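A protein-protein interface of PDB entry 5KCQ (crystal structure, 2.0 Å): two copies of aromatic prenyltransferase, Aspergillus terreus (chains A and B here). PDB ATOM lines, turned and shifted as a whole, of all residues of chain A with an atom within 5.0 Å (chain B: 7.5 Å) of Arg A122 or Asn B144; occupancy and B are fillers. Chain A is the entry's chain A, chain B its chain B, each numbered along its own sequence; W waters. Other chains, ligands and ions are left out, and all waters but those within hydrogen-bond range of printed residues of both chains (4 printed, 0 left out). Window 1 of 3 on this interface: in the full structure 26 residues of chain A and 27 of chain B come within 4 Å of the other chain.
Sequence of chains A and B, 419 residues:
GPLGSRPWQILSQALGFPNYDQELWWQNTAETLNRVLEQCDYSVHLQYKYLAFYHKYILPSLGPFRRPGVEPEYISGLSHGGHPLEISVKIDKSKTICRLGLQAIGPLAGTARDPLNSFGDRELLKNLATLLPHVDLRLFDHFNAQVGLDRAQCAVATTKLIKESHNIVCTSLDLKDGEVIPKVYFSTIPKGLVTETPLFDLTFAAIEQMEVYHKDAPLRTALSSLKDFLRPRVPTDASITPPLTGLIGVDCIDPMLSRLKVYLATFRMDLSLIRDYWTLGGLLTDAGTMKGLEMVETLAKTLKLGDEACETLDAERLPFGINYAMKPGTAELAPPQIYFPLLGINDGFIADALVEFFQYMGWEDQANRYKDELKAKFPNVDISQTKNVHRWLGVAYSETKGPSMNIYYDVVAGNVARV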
ATOM      1  N   PHE A 119      37.863  -7.231   8.097  1.00  0.00           N
ATOM      2  CA  PHE A 119      36.714  -6.281   7.888  1.00  0.00           C
ATOM      3  C   PHE A 119      36.676  -5.593   6.523  1.00  0.00           C
ATOM      4  O   PHE A 119      35.580  -5.169   6.089  1.00  0.00           O
ATOM      5  CB  PHE A 119      36.702  -5.187   8.986  1.00  0.00           C
ATOM      6  CG  PHE A 119      36.858  -5.765  10.337  1.00  0.00           C
ATOM      7  CD1 PHE A 119      35.863  -6.568  10.879  1.00  0.00           C
ATOM      8  CD2 PHE A 119      38.074  -5.665  10.988  1.00  0.00           C
ATOM      9  CE1 PHE A 119      36.044  -7.197  12.129  1.00  0.00           C
ATOM     10  CE2 PHE A 119      38.274  -6.274  12.236  1.00  0.00           C
ATOM     11  CZ  PHE A 119      37.259  -7.069  12.793  1.00  0.00           C
ATOM     12  N   GLY A 120      37.830  -5.406   5.868  1.00  0.00           N
ATOM     13  CA  GLY A 120      37.859  -4.542   4.667  1.00  0.00           C
ATOM     14  C   GLY A 120      36.994  -5.104   3.545  1.00  0.00           C
ATOM     15  O   GLY A 120      36.291  -4.329   2.854  1.00  0.00           O
ATOM     16  N   ASP A 121      37.002  -6.430   3.317  1.00  0.00           N
ATOM     17  CA  ASP A 121      36.303  -6.971   2.102  1.00  0.00           C
ATOM     18  C   ASP A 121      34.803  -6.819   2.236  1.00  0.00           C
ATOM     19  O   ASP A 121      34.107  -6.434   1.298  1.00  0.00           O
ATOM     20  CB  ASP A 121      36.638  -8.444   1.878  1.00  0.00           C
ATOM     21  CG  ASP A 121      38.098  -8.617   1.361  1.00  0.00           C
ATOM     22  OD1 ASP A 121      39.002  -8.576   2.228  1.00  0.00           O
ATOM     23  OD2 ASP A 121      38.314  -8.812   0.127  1.00  0.00           O
ATOM     24  N   ARG A 122      34.308  -7.047   3.450  1.00  0.00           N
ATOM     25  CA  ARG A 122      32.879  -6.805   3.693  1.00  0.00           C
ATOM     26  C   ARG A 122      32.506  -5.338   3.537  1.00  0.00           C
ATOM     27  O   ARG A 122      31.423  -5.006   3.033  1.00  0.00           O
ATOM     28  CB  ARG A 122      32.502  -7.416   5.056  1.00  0.00           C
ATOM     29  CG  ARG A 122      31.070  -7.208   5.534  1.00  0.00           C
ATOM     30  CD  ARG A 122      30.071  -7.762   4.615  1.00  0.00           C
ATOM     31  NE  ARG A 122      28.739  -7.994   5.257  1.00  0.00           N
ATOM     32  CZ  ARG A 122      27.827  -7.040   5.473  1.00  0.00           C
ATOM     33  NH1 ARG A 122      28.106  -5.751   5.281  1.00  0.00           N
ATOM     34  NH2 ARG A 122      26.654  -7.375   5.888  1.00  0.00           N
ATOM     35  N   GLU A 123      33.368  -4.433   3.977  1.00  0.00           N
ATOM     36  CA  GLU A 123      33.072  -3.022   3.840  1.00  0.00           C
ATOM     37  C   GLU A 123      32.954  -2.638   2.333  1.00  0.00           C
ATOM     38  O   GLU A 123      32.051  -1.882   1.940  1.00  0.00           O
ATOM     39  CB  GLU A 123      34.083  -2.086   4.542  1.00  0.00           C
ATOM     40  CG  GLU A 123      33.730  -0.574   4.346  1.00  0.00           C
ATOM     41  CD  GLU A 123      34.739   0.395   4.901  1.00  0.00           C
ATOM     42  OE1 GLU A 123      35.821  -0.051   5.293  1.00  0.00           O
ATOM     43  OE2 GLU A 123      34.483   1.623   4.927  1.00  0.00           O
ATOM     44  N   LEU A 124      33.876  -3.125   1.520  1.00  0.00           N
ATOM     45  CA  LEU A 124      33.800  -2.974   0.082  1.00  0.00           C
ATOM     46  C   LEU A 124      32.498  -3.554  -0.442  1.00  0.00           C
ATOM     47  O   LEU A 124      31.793  -2.945  -1.237  1.00  0.00           O
ATOM     48  CB  LEU A 124      34.993  -3.670  -0.602  1.00  0.00           C
ATOM     49  CG  LEU A 124      34.938  -3.786  -2.134  1.00  0.00           C
ATOM     50  CD1 LEU A 124      34.858  -2.419  -2.777  1.00  0.00           C
ATOM     51  CD2 LEU A 124      36.235  -4.519  -2.591  1.00  0.00           C
ATOM     52  N   LEU A 125      32.186  -4.765  -0.054  1.00  0.00           N
ATOM     53  CA  LEU A 125      30.937  -5.351  -0.495  1.00  0.00           C
ATOM     54  C   LEU A 125      29.681  -4.563  -0.119  1.00  0.00           C
ATOM     55  O   LEU A 125      28.762  -4.472  -0.935  1.00  0.00           O
ATOM     56  CB  LEU A 125      30.852  -6.759   0.013  1.00  0.00           C
ATOM     57  CG  LEU A 125      31.849  -7.666  -0.736  1.00  0.00           C
ATOM     58  CD1 LEU A 125      32.070  -8.973   0.029  1.00  0.00           C
ATOM     59  CD2 LEU A 125      31.293  -7.984  -2.125  1.00  0.00           C
ATOM     60  N   LYS A 126      29.641  -3.989   1.089  1.00  0.00           N
ATOM     61  CA  LYS A 126      28.531  -3.112   1.443  1.00  0.00           C
ATOM     62  C   LYS A 126      28.421  -1.938   0.475  1.00  0.00           C
ATOM     63  O   LYS A 126      27.316  -1.583   0.067  1.00  0.00           O
ATOM     64  CB  LYS A 126      28.747  -2.536   2.830  1.00  0.00           C
ATOM     65  CG  LYS A 126      27.940  -1.272   3.126  1.00  0.00           C
ATOM     66  CD  LYS A 126      28.598  -0.462   4.223  1.00  0.00           C
ATOM     67  CE  LYS A 126      29.220   0.837   3.742  1.00  0.00           C
ATOM     68  NZ  LYS A 126      30.307   1.238   4.671  1.00  0.00           N
ATOM     69  N   LEU A 137      24.698 -10.117  -0.074  1.00  0.00           N
ATOM     70  CA  LEU A 137      25.704 -10.398   0.961  1.00  0.00           C
ATOM     71  C   LEU A 137      25.376 -11.555   1.849  1.00  0.00           C
ATOM     72  O   LEU A 137      26.114 -11.867   2.759  1.00  0.00           O
ATOM     73  CB  LEU A 137      25.835  -9.177   1.853  1.00  0.00           C
ATOM     74  CG  LEU A 137      26.202  -7.857   1.134  1.00  0.00           C
ATOM     75  CD1 LEU A 137      26.707  -6.890   2.167  1.00  0.00           C
ATOM     76  CD2 LEU A 137      27.271  -8.025   0.081  1.00  0.00           C
ATOM     77  N   ARG A 138      24.302 -12.268   1.582  1.00  0.00           N
ATOM     78  CA  ARG A 138      23.919 -13.320   2.541  1.00  0.00           C
ATOM     79  C   ARG A 138      24.909 -14.449   2.627  1.00  0.00           C
ATOM     80  O   ARG A 138      25.215 -14.928   3.713  1.00  0.00           O
ATOM     81  CB  ARG A 138      22.509 -13.781   2.246  1.00  0.00           C
ATOM     82  CG  ARG A 138      21.504 -12.707   2.698  1.00  0.00           C
ATOM     83  CD  ARG A 138      20.084 -12.997   2.221  1.00  0.00           C
ATOM     84  NE  ARG A 138      19.916 -12.928   0.750  1.00  0.00           N
ATOM     85  CZ  ARG A 138      18.710 -12.876   0.185  1.00  0.00           C
ATOM     86  NH1 ARG A 138      17.623 -12.970   0.955  1.00  0.00           N
ATOM     87  NH2 ARG A 138      18.569 -12.752  -1.093  1.00  0.00           N
ATOM     88  N   PHE A 140      28.143 -14.318   1.782  1.00  0.00           N
ATOM     89  CA  PHE A 140      29.278 -13.761   2.459  1.00  0.00           C
ATOM     90  C   PHE A 140      29.108 -13.829   3.976  1.00  0.00           C
ATOM     91  O   PHE A 140      29.989 -14.341   4.708  1.00  0.00           O
ATOM     92  CB  PHE A 140      29.587 -12.337   2.032  1.00  0.00           C
ATOM     93  CG  PHE A 140      30.831 -11.781   2.702  1.00  0.00           C
ATOM     94  CD1 PHE A 140      30.845 -11.460   4.048  1.00  0.00           C
ATOM     95  CD2 PHE A 140      31.987 -11.648   1.999  1.00  0.00           C
ATOM     96  CE1 PHE A 140      31.987 -10.946   4.675  1.00  0.00           C
ATOM     97  CE2 PHE A 140      33.096 -11.088   2.567  1.00  0.00           C
ATOM     98  CZ  PHE A 140      33.130 -10.760   3.900  1.00  0.00           C
ATOM     99  N   ASP A 141      27.972 -13.339   4.463  1.00  0.00           N
ATOM    100  CA  ASP A 141      27.799 -13.275   5.892  1.00  0.00           C
ATOM    101  C   ASP A 141      27.711 -14.644   6.510  1.00  0.00           C
ATOM    102  O   ASP A 141      28.253 -14.884   7.583  1.00  0.00           O
ATOM    103  CB  ASP A 141      26.570 -12.470   6.241  1.00  0.00           C
ATOM    104  CG  ASP A 141      26.767 -10.974   6.007  1.00  0.00           C
ATOM    105  OD1 ASP A 141      27.947 -10.531   5.901  1.00  0.00           O
ATOM    106  OD2 ASP A 141      25.765 -10.201   5.922  1.00  0.00           O
ATOM    107  N   SER B 118      19.820  -1.582   5.656  1.00  0.00           N
ATOM    108  CA  SER B 118      20.389  -2.936   5.814  1.00  0.00           C
ATOM    109  C   SER B 118      21.853  -2.985   6.217  1.00  0.00           C
ATOM    110  O   SER B 118      22.298  -4.012   6.572  1.00  0.00           O
ATOM    111  CB  SER B 118      20.228  -3.746   4.536  1.00  0.00           C
ATOM    112  OG  SER B 118      18.863  -4.011   4.339  1.00  0.00           O
ATOM    113  N   PHE B 119      22.556  -1.866   6.197  1.00  0.00           N
ATOM    114  CA  PHE B 119      24.016  -1.822   6.273  1.00  0.00           C
ATOM    115  C   PHE B 119      24.612  -1.013   7.422  1.00  0.00           C
ATOM    116  O   PHE B 119      25.761  -1.285   7.836  1.00  0.00           O
ATOM    117  CB  PHE B 119      24.619  -1.261   4.963  1.00  0.00           C
ATOM    118  CG  PHE B 119      24.041  -1.916   3.734  1.00  0.00           C
ATOM    119  CD1 PHE B 119      24.250  -3.256   3.493  1.00  0.00           C
ATOM    120  CD2 PHE B 119      23.203  -1.201   2.914  1.00  0.00           C
ATOM    121  CE1 PHE B 119      23.642  -3.884   2.388  1.00  0.00           C
ATOM    122  CE2 PHE B 119      22.572  -1.791   1.825  1.00  0.00           C
ATOM    123  CZ  PHE B 119      22.824  -3.145   1.567  1.00  0.00           C
ATOM    124  N   ARG B 122      25.750  -2.928  10.905  1.00  0.00           N
ATOM    125  CA  ARG B 122      26.964  -3.735  10.761  1.00  0.00           C
ATOM    126  C   ARG B 122      28.214  -2.813  10.579  1.00  0.00           C
ATOM    127  O   ARG B 122      29.293  -3.138  11.025  1.00  0.00           O
ATOM    128  CB  ARG B 122      26.794  -4.732   9.599  1.00  0.00           C
ATOM    129  CG  ARG B 122      27.985  -5.637   9.265  1.00  0.00           C
ATOM    130  CD  ARG B 122      28.492  -6.427  10.433  1.00  0.00           C
ATOM    131  NE  ARG B 122      29.333  -7.599  10.080  1.00  0.00           N
ATOM    132  CZ  ARG B 122      30.590  -7.526   9.678  1.00  0.00           C
ATOM    133  NH1 ARG B 122      31.190  -6.362   9.526  1.00  0.00           N
ATOM    134  NH2 ARG B 122      31.266  -8.618   9.491  1.00  0.00           N
ATOM    135  N   GLU B 123      28.082  -1.707   9.907  1.00  0.00           N
ATOM    136  CA  GLU B 123      29.221  -0.810   9.734  1.00  0.00           C
ATOM    137  C   GLU B 123      29.683  -0.256  11.099  1.00  0.00           C
ATOM    138  O   GLU B 123      30.899  -0.184  11.382  1.00  0.00           O
ATOM    139  CB  GLU B 123      28.948   0.371   8.745  1.00  0.00           C
ATOM    140  CG  GLU B 123      30.180   1.343   8.608  1.00  0.00           C
ATOM    141  CD  GLU B 123      29.901   2.540   7.691  1.00  0.00           C
ATOM    142  OE1 GLU B 123      28.762   2.700   7.214  1.00  0.00           O
ATOM    143  OE2 GLU B 123      30.798   3.356   7.447  1.00  0.00           O
ATOM    144  N   LYS B 126      31.420  -3.115  12.912  1.00  0.00           N
ATOM    145  CA  LYS B 126      32.814  -3.219  12.436  1.00  0.00           C
ATOM    146  C   LYS B 126      33.752  -2.201  13.089  1.00  0.00           C
ATOM    147  O   LYS B 126      34.875  -2.557  13.506  1.00  0.00           O
ATOM    148  CB  LYS B 126      32.896  -2.970  10.923  1.00  0.00           C
ATOM    149  CG  LYS B 126      34.309  -2.638  10.385  1.00  0.00           C
ATOM    150  CD  LYS B 126      34.220  -1.863   9.070  1.00  0.00           C
ATOM    151  CE  LYS B 126      34.620  -0.411   9.159  1.00  0.00           C
ATOM    152  NZ  LYS B 126      33.945   0.369   8.113  1.00  0.00           N
ATOM    153  N   LEU B 137      31.481 -10.632  16.027  1.00  0.00           N
ATOM    154  CA  LEU B 137      30.434 -10.383  15.016  1.00  0.00           C
ATOM    155  C   LEU B 137      29.821 -11.677  14.429  1.00  0.00           C
ATOM    156  O   LEU B 137      29.047 -11.602  13.508  1.00  0.00           O
ATOM    157  CB  LEU B 137      31.043  -9.589  13.859  1.00  0.00           C
ATOM    158  CG  LEU B 137      31.634  -8.207  14.181  1.00  0.00           C
ATOM    159  CD1 LEU B 137      31.809  -7.373  12.904  1.00  0.00           C
ATOM    160  CD2 LEU B 137      30.781  -7.426  15.148  1.00  0.00           C
ATOM    161  N   ARG B 138      30.223 -12.849  14.896  1.00  0.00           N
ATOM    162  CA  ARG B 138      29.822 -14.033  14.200  1.00  0.00           C
ATOM    163  C   ARG B 138      28.320 -14.320  14.272  1.00  0.00           C
ATOM    164  O   ARG B 138      27.737 -14.742  13.260  1.00  0.00           O
ATOM    165  CB  ARG B 138      30.645 -15.198  14.678  1.00  0.00           C
ATOM    166  CG  ARG B 138      32.027 -15.120  13.997  1.00  0.00           C
ATOM    167  CD  ARG B 138      33.010 -16.074  14.575  1.00  0.00           C
ATOM    168  NE  ARG B 138      33.312 -15.837  15.997  1.00  0.00           N
ATOM    169  CZ  ARG B 138      34.237 -16.547  16.617  1.00  0.00           C
ATOM    170  NH1 ARG B 138      34.908 -17.443  15.915  1.00  0.00           N
ATOM    171  NH2 ARG B 138      34.506 -16.382  17.893  1.00  0.00           N
ATOM    172  N   LEU B 139      27.696 -14.053  15.426  1.00  0.00           N
ATOM    173  CA  LEU B 139      26.268 -14.248  15.496  1.00  0.00           C
ATOM    174  C   LEU B 139      25.503 -13.153  14.736  1.00  0.00           C
ATOM    175  O   LEU B 139      24.423 -13.407  14.196  1.00  0.00           O
ATOM    176  CB  LEU B 139      25.786 -14.384  16.949  1.00  0.00           C
ATOM    177  CG  LEU B 139      26.239 -15.657  17.681  1.00  0.00           C
ATOM    178  CD1 LEU B 139      25.785 -15.599  19.137  1.00  0.00           C
ATOM    179  CD2 LEU B 139      25.654 -16.880  16.968  1.00  0.00           C
ATOM    180  N   PHE B 140      26.018 -11.928  14.735  1.00  0.00           N
ATOM    181  CA  PHE B 140      25.430 -10.932  13.907  1.00  0.00           C
ATOM    182  C   PHE B 140      25.381 -11.455  12.482  1.00  0.00           C
ATOM    183  O   PHE B 140      24.363 -11.343  11.788  1.00  0.00           O
ATOM    184  CB  PHE B 140      26.176  -9.578  13.979  1.00  0.00           C
ATOM    185  CG  PHE B 140      25.564  -8.507  13.134  1.00  0.00           C
ATOM    186  CD1 PHE B 140      25.669  -8.518  11.755  1.00  0.00           C
ATOM    187  CD2 PHE B 140      24.821  -7.481  13.712  1.00  0.00           C
ATOM    188  CE1 PHE B 140      25.054  -7.579  10.968  1.00  0.00           C
ATOM    189  CE2 PHE B 140      24.218  -6.505  12.905  1.00  0.00           C
ATOM    190  CZ  PHE B 140      24.309  -6.562  11.551  1.00  0.00           C
ATOM    191  N   ASP B 141      26.526 -11.919  12.002  1.00  0.00           N
ATOM    192  CA  ASP B 141      26.614 -12.260  10.613  1.00  0.00           C
ATOM    193  C   ASP B 141      25.730 -13.493  10.347  1.00  0.00           C
ATOM    194  O   ASP B 141      25.111 -13.595   9.306  1.00  0.00           O
ATOM    195  CB  ASP B 141      28.016 -12.518  10.242  1.00  0.00           C
ATOM    196  CG  ASP B 141      28.852 -11.189  10.135  1.00  0.00           C
ATOM    197  OD1 ASP B 141      28.262 -10.115  10.027  1.00  0.00           O
ATOM    198  OD2 ASP B 141      30.113 -11.277  10.027  1.00  0.00           O
ATOM    199  N   HIS B 142      25.721 -14.415  11.275  1.00  0.00           N
ATOM    200  CA  HIS B 142      24.813 -15.566  11.120  1.00  0.00           C
ATOM    201  C   HIS B 142      23.359 -15.137  10.886  1.00  0.00           C
ATOM    202  O   HIS B 142      22.700 -15.471   9.858  1.00  0.00           O
ATOM    203  CB  HIS B 142      24.917 -16.481  12.341  1.00  0.00           C
ATOM    204  CG  HIS B 142      23.918 -17.586  12.274  1.00  0.00           C
ATOM    205  ND1 HIS B 142      24.089 -18.674  11.462  1.00  0.00           N
ATOM    206  CD2 HIS B 142      22.653 -17.651  12.732  1.00  0.00           C
ATOM    207  CE1 HIS B 142      23.000 -19.422  11.496  1.00  0.00           C
ATOM    208  NE2 HIS B 142      22.098 -18.806  12.232  1.00  0.00           N
ATOM    209  N   PHE B 143      22.804 -14.343  11.815  1.00  0.00           N
ATOM    210  CA  PHE B 143      21.416 -13.910  11.643  1.00  0.00           C
ATOM    211  C   PHE B 143      21.181 -12.932  10.500  1.00  0.00           C
ATOM    212  O   PHE B 143      20.140 -12.989   9.822  1.00  0.00           O
ATOM    213  CB  PHE B 143      20.849 -13.439  12.988  1.00  0.00           C
ATOM    214  CG  PHE B 143      20.558 -14.579  13.880  1.00  0.00           C
ATOM    215  CD1 PHE B 143      19.511 -15.473  13.556  1.00  0.00           C
ATOM    216  CD2 PHE B 143      21.359 -14.858  14.945  1.00  0.00           C
ATOM    217  CE1 PHE B 143      19.285 -16.613  14.335  1.00  0.00           C
ATOM    218  CE2 PHE B 143      21.102 -15.980  15.750  1.00  0.00           C
ATOM    219  CZ  PHE B 143      20.097 -16.879  15.433  1.00  0.00           C
ATOM    220  N   ASN B 144      22.164 -12.130  10.156  1.00  0.00           N
ATOM    221  CA  ASN B 144      21.996 -11.220   9.010  1.00  0.00           C
ATOM    222  C   ASN B 144      21.875 -12.124   7.745  1.00  0.00           C
ATOM    223  O   ASN B 144      21.161 -11.812   6.777  1.00  0.00           O
ATOM    224  CB  ASN B 144      23.182 -10.260   8.902  1.00  0.00           C
ATOM    225  CG  ASN B 144      22.887  -9.031   8.094  1.00  0.00           C
ATOM    226  OD1 ASN B 144      23.700  -8.577   7.262  1.00  0.00           O
ATOM    227  ND2 ASN B 144      21.721  -8.510   8.264  1.00  0.00           N
ATOM    228  N   ALA B 145      22.613 -13.215   7.756  1.00  0.00           N
ATOM    229  CA  ALA B 145      22.568 -14.149   6.614  1.00  0.00           C
ATOM    230  C   ALA B 145      21.177 -14.845   6.524  1.00  0.00           C
ATOM    231  O   ALA B 145      20.661 -15.046   5.448  1.00  0.00           O
ATOM    232  CB  ALA B 145      23.655 -15.191   6.722  1.00  0.00           C
ATOM    233  N   GLN B 146      20.597 -15.159   7.641  1.00  0.00           N
ATOM    234  CA  GLN B 146      19.360 -15.925   7.654  1.00  0.00           C
ATOM    235  C   GLN B 146      18.151 -15.040   7.487  1.00  0.00           C
ATOM    236  O   GLN B 146      17.183 -15.467   6.891  1.00  0.00           O
ATOM    237  CB  GLN B 146      19.179 -16.653   9.000  1.00  0.00           C
ATOM    238  CG  GLN B 146      20.329 -17.526   9.415  1.00  0.00           C
ATOM    239  CD  GLN B 146      20.712 -18.497   8.337  1.00  0.00           C
ATOM    240  OE1 GLN B 146      21.882 -18.575   7.888  1.00  0.00           O
ATOM    241  NE2 GLN B 146      19.733 -19.265   7.930  1.00  0.00           N
ATOM    242  N   VAL B 147      18.147 -13.826   8.067  1.00  0.00           N
ATOM    243  CA  VAL B 147      16.953 -12.976   7.894  1.00  0.00           C
ATOM    244  C   VAL B 147      17.072 -11.711   7.040  1.00  0.00           C
ATOM    245  O   VAL B 147      16.067 -11.005   6.841  1.00  0.00           O
ATOM    246  CB  VAL B 147      16.257 -12.655   9.216  1.00  0.00           C
ATOM    247  CG1 VAL B 147      16.018 -13.952   9.973  1.00  0.00           C
ATOM    248  CG2 VAL B 147      17.045 -11.673  10.032  1.00  0.00           C
ATOM    249  N   GLY B 148      18.277 -11.397   6.580  1.00  0.00           N
ATOM    250  CA  GLY B 148      18.472 -10.179   5.797  1.00  0.00           C
ATOM    251  C   GLY B 148      17.877 -10.442   4.421  1.00  0.00           C
ATOM    252  O   GLY B 148      17.581 -11.585   4.064  1.00  0.00           O
ATOM    253  N   LEU B 149      17.696  -9.383   3.643  1.00  0.00           N
ATOM    254  CA  LEU B 149      17.036  -9.472   2.336  1.00  0.00           C
ATOM    255  C   LEU B 149      17.860  -8.737   1.304  1.00  0.00           C
ATOM    256  O   LEU B 149      18.516  -7.752   1.668  1.00  0.00           O
ATOM    257  CB  LEU B 149      15.695  -8.740   2.448  1.00  0.00           C
ATOM    258  CG  LEU B 149      14.604  -9.343   3.339  1.00  0.00           C
ATOM    259  CD1 LEU B 149      13.370  -8.518   3.338  1.00  0.00           C
ATOM    260  CD2 LEU B 149      14.342 -10.762   2.829  1.00  0.00           C
ATOM    261  N   ILE B 168      15.422  -3.917   9.622  1.00  0.00           N
ATOM    262  CA  ILE B 168      15.749  -5.317   9.828  1.00  0.00           C
ATOM    263  C   ILE B 168      16.554  -5.526  11.095  1.00  0.00           C
ATOM    264  O   ILE B 168      16.452  -6.581  11.673  1.00  0.00           O
ATOM    265  CB  ILE B 168      16.605  -5.865   8.675  1.00  0.00           C
ATOM    266  CG1 ILE B 168      15.794  -5.984   7.401  1.00  0.00           C
ATOM    267  CG2 ILE B 168      17.150  -7.251   9.013  1.00  0.00           C
ATOM    268  CD1 ILE B 168      15.420  -7.394   7.029  1.00  0.00           C
ATOM    269  N   VAL B 169      17.353  -4.548  11.544  1.00  0.00           N
ATOM    270  CA  VAL B 169      18.167  -4.737  12.740  1.00  0.00           C
ATOM    271  C   VAL B 169      18.103  -3.495  13.622  1.00  0.00           C
ATOM    272  O   VAL B 169      17.817  -2.377  13.115  1.00  0.00           O
ATOM    273  CB  VAL B 169      19.578  -5.260  12.308  1.00  0.00           C
ATOM    274  CG1 VAL B 169      20.307  -4.280  11.472  1.00  0.00           C
ATOM    275  CG2 VAL B 169      20.457  -5.564  13.522  1.00  0.00           C
ATOM    276  N   PHE B 186      17.251  -8.768  15.430  1.00  0.00           N
ATOM    277  CA  PHE B 186      16.892  -8.892  14.048  1.00  0.00           C
ATOM    278  C   PHE B 186      15.387  -9.106  13.966  1.00  0.00           C
ATOM    279  O   PHE B 186      14.804  -9.945  14.678  1.00  0.00           O
ATOM    280  CB  PHE B 186      17.618 -10.098  13.432  1.00  0.00           C
ATOM    281  CG  PHE B 186      19.084  -9.861  13.169  1.00  0.00           C
ATOM    282  CD1 PHE B 186      19.477  -9.350  11.967  1.00  0.00           C
ATOM    283  CD2 PHE B 186      20.049 -10.140  14.121  1.00  0.00           C
ATOM    284  CE1 PHE B 186      20.809  -9.068  11.726  1.00  0.00           C
ATOM    285  CE2 PHE B 186      21.387  -9.861  13.870  1.00  0.00           C
ATOM    286  CZ  PHE B 186      21.755  -9.346  12.651  1.00  0.00           C
HETATM  287  O   HOH W   1      23.813  -6.061   5.472  1.00  0.00           O
HETATM  288  O   HOH W   2      23.319 -10.876   4.814  1.00  0.00           O
HETATM  289  O   HOH W   3      27.443  -3.096   6.337  1.00  0.00           O
HETATM  290  O   HOH W   4      33.241  -5.152   7.762  1.00  0.00           O
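NH2 of Arg A122 sits at hydrogen-bond distance from OD1 of Asn B144 (3.5 Å). OE1 of Glu A123 lies within salt-bridge range of NZ of Lys B126. The guanidinium group (NH1) of Arg A138 lies within hydrogen-bond range of the backbone carbonyl oxygen (O) of Gly B148 (3.4 Å). The side-chain carboxylate of Asp A141 lies close to the side-chain amide oxygen of Asn B144 (2.9 Å). The side-chain amino group of Lys A126 lies within salt-bridge range of the side-chain carboxylate of Glu B123, at 3.3 Å.
The guanidinium group (NE) of Arg B122 lies within salt-bridge range of the side-chain carboxylate (OD1) of Asp B141. NE of Arg A122 is in salt-bridge range of OD1 of Asp A141 (2.7 Å).
CB of Phe A119 touches CG of Lys B126 (3.8 Å). CG of Arg B122 touches NH1 of Arg A122 (3.99 Å). CG of Lys A126 touches CB of Phe B119 (3.8 Å). Arg A138 touches Ala B145 (O to CB, 3.4 Å). Arg A138 touches Leu B149 (NH1 to CA, 3.8 Å). Asp A141 touches Asp B141.
Of the printed residues of chain B, Arg A122 touches Arg B122 and Asn B144. Printed residues of chain B within 4 Å of Asp A141: Asp B141 and Asn B144. Of the printed residues of chain A, Lys B126 touches Phe A119 and Glu A123. Asn B144 touches just these residues of chain A: Arg A122 and Asp A141. Of the printed residues of chain A, Ala B145 touches Arg A138. Val B147 touches none of the printed residues of chain A. Printed residues of chain A within 4 Å of Gly B148: Arg A138 (3.4 Å). The nearest printed residue of chain B that does not touch Arg A122 is Phe B119 (4.9 Å). The nearest residue of chain A that does not touch Asn B144 is Arg A138 (4.2 Å). The nearest printed residue of chain B that does not touch Phe A119 is Leu B137 (4.3 Å).
Hydrophobic or aromatic side chains of chain B that line the printed part of chain A: Phe B119 and Ala B145. Along chain B the printed residues that touch a printed residue of chain A span positions 119 to 149. Hydrophobic or aromatic side chains of chain A that line the printed part of chain B: Phe A119. Along chain A the printed residues that touch a printed residue of chain B span positions 119 to 141.
Phe A119 touches Lys B126, and with the chains exchanged Lys A126 touches Phe B119. Arg B122 touches its own counterpart, Arg A122. Glu A123 touches Lys B126, and with the chains exchanged Lys A126 touches Glu B123. Asp A141 touches its own counterpart, Asp B141. 8 positions are printed for both chains.
Water W2 lies within hydrogen-bond range of the side-chain carboxylate of Asp A141 (2.8 Å) and the backbone carbonyl oxygen of Asn B144 (3.1 Å). Water W1 lies within hydrogen-bond range of O of Ser B118, OD1 of Asn B144 and NH2 of Arg A122. Water W4 lies within hydrogen-bond range of the backbone carbonyl oxygen of Phe A119 (2.9 Å) and the guanidinium group of Arg B122 (3.0 Å). Water W3 bridges the backbone carbonyl oxygen of Phe B119 (2.9 Å) and the guanidinium group of Arg A122 (2.9 Å).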
